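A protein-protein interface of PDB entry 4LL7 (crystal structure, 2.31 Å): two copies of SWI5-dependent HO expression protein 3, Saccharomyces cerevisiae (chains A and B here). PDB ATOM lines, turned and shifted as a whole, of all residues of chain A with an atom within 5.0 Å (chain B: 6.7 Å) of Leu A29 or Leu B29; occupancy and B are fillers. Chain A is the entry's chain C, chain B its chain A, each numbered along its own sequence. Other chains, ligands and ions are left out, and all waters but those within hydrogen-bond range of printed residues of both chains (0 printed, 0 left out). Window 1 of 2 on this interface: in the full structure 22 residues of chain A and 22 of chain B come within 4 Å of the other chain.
Among the printed residues, pairs that only touch across the chains: Gln A25 with Ser B26, Ser A26 with Gln B25, Leu A29 with Ser B26, Leu A29 with Leu B29 and Lys A32 with Leu B33.
Asn A28 touches none of the printed residues of chain B. Of chain B, only Ser B26 and Leu B29 come within 4 Å of Leu A29. Printed residues of chain B within 4 Å of Lys A32: Leu B33. Printed residues of chain A within 4 Å of Gln B25: Ser A26 (3.5 Å). Of chain A, only Leu A29 (3.3 Å) comes within 4 Å of Leu B29. Of the printed residues of chain A, Leu B33 touches Lys A32. The nearest residue of chain A that does not touch Leu B29 is Ser A26 (4.4 Å). The nearest printed residue of chain B that does not touch Ser A26 is Ser B26 (4.2 Å).
Of the 13 printed residues of chain B, 4 touch a printed residue of chain A. Along chain A the printed residues that touch a printed residue of chain B span positions 25 to 32. Among the printed residues, no Asp or Glu carboxylate lies within 4 Å of a Lys or Arg side-chain nitrogen of the other chain.
Gln A25 touches Ser B26, and with the chains exchanged Ser A26 touches Gln B25. Leu A29 touches Ser B26, but with the chains exchanged Ser A26 does not touch Leu B29 (4.4 Å). Leu A29 touches its own counterpart, Leu B29. Lys A32 touches Leu B33, but with the chains exchanged Leu A33 does not touch Lys B32 (4.8 Å). Of the 5 pairs that touch across the chains among the printed residues, 3 have their exchanged pair printed and touching as well.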
ATOM      1  N   GLN A  25      10.512 -21.004  21.582  1.00  0.00           N
ATOM      2  CA  GLN A  25      10.162 -21.439  22.927  1.00  0.00           C
ATOM      3  C   GLN A  25       9.624 -20.253  23.713  1.00  0.00           C
ATOM      4  O   GLN A  25       8.642 -20.375  24.443  1.00  0.00           O
ATOM      5  CB  GLN A  25      11.378 -22.019  23.655  1.00  0.00           C
ATOM      6  CG  GLN A  25      11.795 -23.402  23.186  1.00  0.00           C
ATOM      7  CD  GLN A  25      12.586 -24.149  24.244  1.00  0.00           C
ATOM      8  OE1 GLN A  25      13.580 -23.643  24.765  1.00  0.00           O
ATOM      9  NE2 GLN A  25      12.148 -25.362  24.565  1.00  0.00           N
ATOM     10  N   SER A  26      10.277 -19.105  23.561  1.00  0.00           N
ATOM     11  CA  SER A  26       9.856 -17.890  24.245  1.00  0.00           C
ATOM     12  C   SER A  26       8.418 -17.562  23.858  1.00  0.00           C
ATOM     13  O   SER A  26       7.599 -17.202  24.704  1.00  0.00           O
ATOM     14  CB  SER A  26      10.773 -16.727  23.863  1.00  0.00           C
ATOM     15  OG  SER A  26      10.258 -15.496  24.339  1.00  0.00           O
ATOM     16  N   GLN A  27       8.124 -17.692  22.568  1.00  0.00           N
ATOM     17  CA  GLN A  27       6.794 -17.432  22.031  1.00  0.00           C
ATOM     18  C   GLN A  27       5.783 -18.382  22.664  1.00  0.00           C
ATOM     19  O   GLN A  27       4.689 -17.974  23.055  1.00  0.00           O
ATOM     20  CB  GLN A  27       6.805 -17.632  20.514  1.00  0.00           C
ATOM     21  CG  GLN A  27       5.430 -17.674  19.860  1.00  0.00           C
ATOM     22  CD  GLN A  27       4.815 -16.302  19.690  1.00  0.00           C
ATOM     23  OE1 GLN A  27       5.409 -15.418  19.073  1.00  0.00           O
ATOM     24  NE2 GLN A  27       3.613 -16.119  20.228  1.00  0.00           N
ATOM     25  N   ASN A  28       6.158 -19.654  22.751  1.00  0.00           N
ATOM     26  CA  ASN A  28       5.292 -20.668  23.336  1.00  0.00           C
ATOM     27  C   ASN A  28       5.069 -20.380  24.815  1.00  0.00           C
ATOM     28  O   ASN A  28       3.951 -20.503  25.318  1.00  0.00           O
ATOM     29  CB  ASN A  28       5.912 -22.054  23.168  1.00  0.00           C
ATOM     30  CG  ASN A  28       5.037 -23.152  23.731  1.00  0.00           C
ATOM     31  OD1 ASN A  28       3.920 -23.371  23.262  1.00  0.00           O
ATOM     32  ND2 ASN A  28       5.537 -23.846  24.745  1.00  0.00           N
ATOM     33  N   LEU A  29       6.138 -19.999  25.508  1.00  0.00           N
ATOM     34  CA  LEU A  29       6.055 -19.688  26.930  1.00  0.00           C
ATOM     35  C   LEU A  29       5.154 -18.472  27.132  1.00  0.00           C
ATOM     36  O   LEU A  29       4.366 -18.423  28.076  1.00  0.00           O
ATOM     37  CB  LEU A  29       7.455 -19.415  27.494  1.00  0.00           C
ATOM     38  CG  LEU A  29       8.473 -20.545  27.301  1.00  0.00           C
ATOM     39  CD1 LEU A  29       9.806 -20.152  27.908  1.00  0.00           C
ATOM     40  CD2 LEU A  29       7.957 -21.822  27.939  1.00  0.00           C
ATOM     41  N   LEU A  30       5.272 -17.496  26.235  1.00  0.00           N
ATOM     42  CA  LEU A  30       4.457 -16.287  26.296  1.00  0.00           C
ATOM     43  C   LEU A  30       2.982 -16.636  26.130  1.00  0.00           C
ATOM     44  O   LEU A  30       2.126 -16.103  26.837  1.00  0.00           O
ATOM     45  CB  LEU A  30       4.870 -15.313  25.192  1.00  0.00           C
ATOM     46  CG  LEU A  30       3.876 -14.186  24.894  1.00  0.00           C
ATOM     47  CD1 LEU A  30       3.846 -13.198  26.051  1.00  0.00           C
ATOM     48  CD2 LEU A  30       4.272 -13.489  23.605  1.00  0.00           C
ATOM     49  N   SER A  31       2.691 -17.525  25.183  1.00  0.00           N
ATOM     50  CA  SER A  31       1.319 -17.952  24.931  1.00  0.00           C
ATOM     51  C   SER A  31       0.750 -18.662  26.150  1.00  0.00           C
ATOM     52  O   SER A  31      -0.418 -18.482  26.495  1.00  0.00           O
ATOM     53  CB  SER A  31       1.254 -18.888  23.720  1.00  0.00           C
ATOM     54  OG  SER A  31       1.132 -18.156  22.512  1.00  0.00           O
ATOM     55  N   LYS A  32       1.580 -19.473  26.797  1.00  0.00           N
ATOM     56  CA  LYS A  32       1.154 -20.201  27.983  1.00  0.00           C
ATOM     57  C   LYS A  32       0.839 -19.218  29.107  1.00  0.00           C
ATOM     58  O   LYS A  32      -0.121 -19.405  29.854  1.00  0.00           O
ATOM     59  CB  LYS A  32       2.243 -21.184  28.425  1.00  0.00           C
ATOM     60  CG  LYS A  32       2.554 -22.257  27.387  1.00  0.00           C
ATOM     61  CD  LYS A  32       1.290 -22.991  26.964  1.00  0.00           C
ATOM     62  CE  LYS A  32       1.536 -23.885  25.760  1.00  0.00           C
ATOM     63  NZ  LYS A  32       0.280 -24.546  25.306  1.00  0.00           N
ATOM     64  N   LEU A  33       1.647 -18.167  29.217  1.00  0.00           N
ATOM     65  CA  LEU A  33       1.439 -17.150  30.242  1.00  0.00           C
ATOM     66  C   LEU A  33       0.120 -16.436  29.977  1.00  0.00           C
ATOM     67  O   LEU A  33      -0.633 -16.130  30.903  1.00  0.00           O
ATOM     68  CB  LEU A  33       2.584 -16.134  30.227  1.00  0.00           C
ATOM     69  CG  LEU A  33       2.475 -14.967  31.214  1.00  0.00           C
ATOM     70  CD1 LEU A  33       2.424 -15.497  32.641  1.00  0.00           C
ATOM     71  CD2 LEU A  33       3.661 -14.034  31.034  1.00  0.00           C
ATOM     72  N   LEU B  22      17.957 -14.787  24.940  1.00  0.00           N
ATOM     73  CA  LEU B  22      16.819 -15.672  24.724  1.00  0.00           C
ATOM     74  C   LEU B  22      16.772 -16.830  25.717  1.00  0.00           C
ATOM     75  O   LEU B  22      15.699 -17.200  26.191  1.00  0.00           O
ATOM     76  CB  LEU B  22      16.840 -16.221  23.294  1.00  0.00           C
ATOM     77  CG  LEU B  22      16.312 -15.311  22.179  1.00  0.00           C
ATOM     78  CD1 LEU B  22      17.018 -13.965  22.206  1.00  0.00           C
ATOM     79  CD2 LEU B  22      16.511 -15.999  20.841  1.00  0.00           C
ATOM     80  N   THR B  24      18.138 -16.967  28.839  1.00  0.00           N
ATOM     81  CA  THR B  24      17.788 -16.465  30.165  1.00  0.00           C
ATOM     82  C   THR B  24      16.290 -16.184  30.167  1.00  0.00           C
ATOM     83  O   THR B  24      15.625 -16.285  31.198  1.00  0.00           O
ATOM     84  CB  THR B  24      18.534 -15.155  30.525  1.00  0.00           C
ATOM     85  OG1 THR B  24      18.201 -14.130  29.578  1.00  0.00           O
ATOM     86  CG2 THR B  24      20.041 -15.382  30.539  1.00  0.00           C
ATOM     87  N   GLN B  25      15.761 -15.837  28.997  1.00  0.00           N
ATOM     88  CA  GLN B  25      14.342 -15.550  28.863  1.00  0.00           C
ATOM     89  C   GLN B  25      13.548 -16.825  29.123  1.00  0.00           C
ATOM     90  O   GLN B  25      12.640 -16.843  29.950  1.00  0.00           O
ATOM     91  CB  GLN B  25      14.050 -15.003  27.463  1.00  0.00           C
ATOM     92  CG  GLN B  25      12.624 -14.532  27.260  1.00  0.00           C
ATOM     93  CD  GLN B  25      12.541 -13.319  26.352  1.00  0.00           C
ATOM     94  OE1 GLN B  25      13.536 -12.903  25.760  1.00  0.00           O
ATOM     95  NE2 GLN B  25      11.349 -12.746  26.238  1.00  0.00           N
ATOM     96  N   SER B  26      13.901 -17.898  28.426  1.00  0.00           N
ATOM     97  CA  SER B  26      13.215 -19.166  28.623  1.00  0.00           C
ATOM     98  C   SER B  26      13.454 -19.669  30.041  1.00  0.00           C
ATOM     99  O   SER B  26      12.878 -20.671  30.460  1.00  0.00           O
ATOM    100  CB  SER B  26      13.707 -20.194  27.610  1.00  0.00           C
ATOM    101  OG  SER B  26      13.345 -19.799  26.298  1.00  0.00           O
ATOM    102  N   GLN B  27      14.315 -18.971  30.776  1.00  0.00           N
ATOM    103  CA  GLN B  27      14.611 -19.336  32.157  1.00  0.00           C
ATOM    104  C   GLN B  27      13.578 -18.642  33.021  1.00  0.00           C
ATOM    105  O   GLN B  27      12.889 -19.271  33.823  1.00  0.00           O
ATOM    106  CB  GLN B  27      15.990 -18.832  32.591  1.00  0.00           C
ATOM    107  CG  GLN B  27      17.140 -19.151  31.660  1.00  0.00           C
ATOM    108  CD  GLN B  27      18.062 -20.218  32.203  1.00  0.00           C
ATOM    109  OE1 GLN B  27      17.961 -21.388  31.835  1.00  0.00           O
ATOM    110  NE2 GLN B  27      18.968 -19.820  33.091  1.00  0.00           N
ATOM    111  N   ASN B  28      13.478 -17.330  32.839  1.00  0.00           N
ATOM    112  CA  ASN B  28      12.555 -16.527  33.616  1.00  0.00           C
ATOM    113  C   ASN B  28      11.092 -16.921  33.420  1.00  0.00           C
ATOM    114  O   ASN B  28      10.282 -16.747  34.329  1.00  0.00           O
ATOM    115  CB  ASN B  28      12.767 -15.024  33.323  1.00  0.00           C
ATOM    116  CG  ASN B  28      11.825 -14.471  32.254  1.00  0.00           C
ATOM    117  OD1 ASN B  28      11.480 -13.289  32.277  1.00  0.00           O
ATOM    118  ND2 ASN B  28      11.426 -15.309  31.313  1.00  0.00           N
ATOM    119  N   LEU B  29      10.760 -17.479  32.256  1.00  0.00           N
ATOM    120  CA  LEU B  29       9.377 -17.862  31.975  1.00  0.00           C
ATOM    121  C   LEU B  29       9.029 -19.265  32.458  1.00  0.00           C
ATOM    122  O   LEU B  29       7.896 -19.516  32.866  1.00  0.00           O
ATOM    123  CB  LEU B  29       9.072 -17.756  30.473  1.00  0.00           C
ATOM    124  CG  LEU B  29       9.479 -16.510  29.675  1.00  0.00           C
ATOM    125  CD1 LEU B  29      10.289 -16.981  28.484  1.00  0.00           C
ATOM    126  CD2 LEU B  29       8.272 -15.703  29.202  1.00  0.00           C
ATOM    127  N   LEU B  30       9.979 -20.193  32.405  1.00  0.00           N
ATOM    128  CA  LEU B  30       9.664 -21.528  32.883  1.00  0.00           C
ATOM    129  C   LEU B  30       9.556 -21.430  34.400  1.00  0.00           C
ATOM    130  O   LEU B  30       9.091 -22.354  35.061  1.00  0.00           O
ATOM    131  CB  LEU B  30      10.734 -22.550  32.508  1.00  0.00           C
ATOM    132  CG  LEU B  30      10.098 -23.939  32.642  1.00  0.00           C
ATOM    133  CD1 LEU B  30       9.428 -24.312  31.322  1.00  0.00           C
ATOM    134  CD2 LEU B  30      11.133 -24.978  33.034  1.00  0.00           C
ATOM    135  N   SER B  31       9.990 -20.289  34.935  1.00  0.00           N
ATOM    136  CA  SER B  31       9.934 -20.030  36.368  1.00  0.00           C
ATOM    137  C   SER B  31       8.677 -19.255  36.726  1.00  0.00           C
ATOM    138  O   SER B  31       8.376 -19.063  37.900  1.00  0.00           O
ATOM    139  CB  SER B  31      11.170 -19.258  36.837  1.00  0.00           C
ATOM    140  OG  SER B  31      12.199 -20.151  37.241  1.00  0.00           O
ATOM    141  N   LYS B  32       7.960 -18.789  35.711  1.00  0.00           N
ATOM    142  CA  LYS B  32       6.705 -18.081  35.933  1.00  0.00           C
ATOM    143  C   LYS B  32       5.576 -19.071  35.692  1.00  0.00           C
ATOM    144  O   LYS B  32       4.794 -19.374  36.595  1.00  0.00           O
ATOM    145  CB  LYS B  32       6.555 -16.904  34.976  1.00  0.00           C
ATOM    146  CG  LYS B  32       7.271 -15.666  35.436  1.00  0.00           C
ATOM    147  CD  LYS B  32       6.873 -14.483  34.588  1.00  0.00           C
ATOM    148  CE  LYS B  32       7.593 -13.237  35.058  1.00  0.00           C
ATOM    149  NZ  LYS B  32       7.435 -12.102  34.106  1.00  0.00           N
ATOM    150  N   LEU B  33       5.501 -19.579  34.467  1.00  0.00           N
ATOM    151  CA  LEU B  33       4.471 -20.542  34.112  1.00  0.00           C
ATOM    152  C   LEU B  33       4.262 -21.487  35.294  1.00  0.00           C
ATOM    153  O   LEU B  33       3.132 -21.875  35.592  1.00  0.00           O
ATOM    154  CB  LEU B  33       4.894 -21.320  32.866  1.00  0.00           C
ATOM    155  CG  LEU B  33       3.827 -22.078  32.070  1.00  0.00           C
ATOM    156  CD1 LEU B  33       4.448 -22.565  30.769  1.00  0.00           C
ATOM    157  CD2 LEU B  33       3.273 -23.245  32.878  1.00  0.00           C
ATOM    158  N   GLU B  34       5.353 -21.843  35.973  1.00  0.00           N
ATOM    159  CA  GLU B  34       5.276 -22.720  37.139  1.00  0.00           C
ATOM    160  C   GLU B  34       4.532 -21.992  38.254  1.00  0.00           C
ATOM    161  O   GLU B  34       3.671 -22.568  38.920  1.00  0.00           O
ATOM    162  CB  GLU B  34       6.676 -23.104  37.628  1.00  0.00           C
ATOM    163  CG  GLU B  34       7.479 -23.938  36.647  1.00  0.00           C
ATOM    164  CD  GLU B  34       8.822 -24.372  37.214  1.00  0.00           C
ATOM    165  OE1 GLU B  34       8.867 -25.403  37.920  1.00  0.00           O
ATOM    166  OE2 GLU B  34       9.828 -23.673  36.966  1.00  0.00           O
ATOM    167  N   LEU B  35       4.875 -20.723  38.460  1.00  0.00           N
ATOM    168  CA  LEU B  35       4.219 -19.910  39.475  1.00  0.00           C
ATOM    169  C   LEU B  35       2.729 -19.812  39.163  1.00  0.00           C
ATOM    170  O   LEU B  35       1.891 -19.936  40.056  1.00  0.00           O
ATOM    171  CB  LEU B  35       4.825 -18.503  39.516  1.00  0.00           C
ATOM    172  CG  LEU B  35       6.262 -18.354  40.026  1.00  0.00           C
ATOM    173  CD1 LEU B  35       6.644 -16.880  40.042  1.00  0.00           C
ATOM    174  CD2 LEU B  35       6.380 -18.945  41.423  1.00  0.00           C
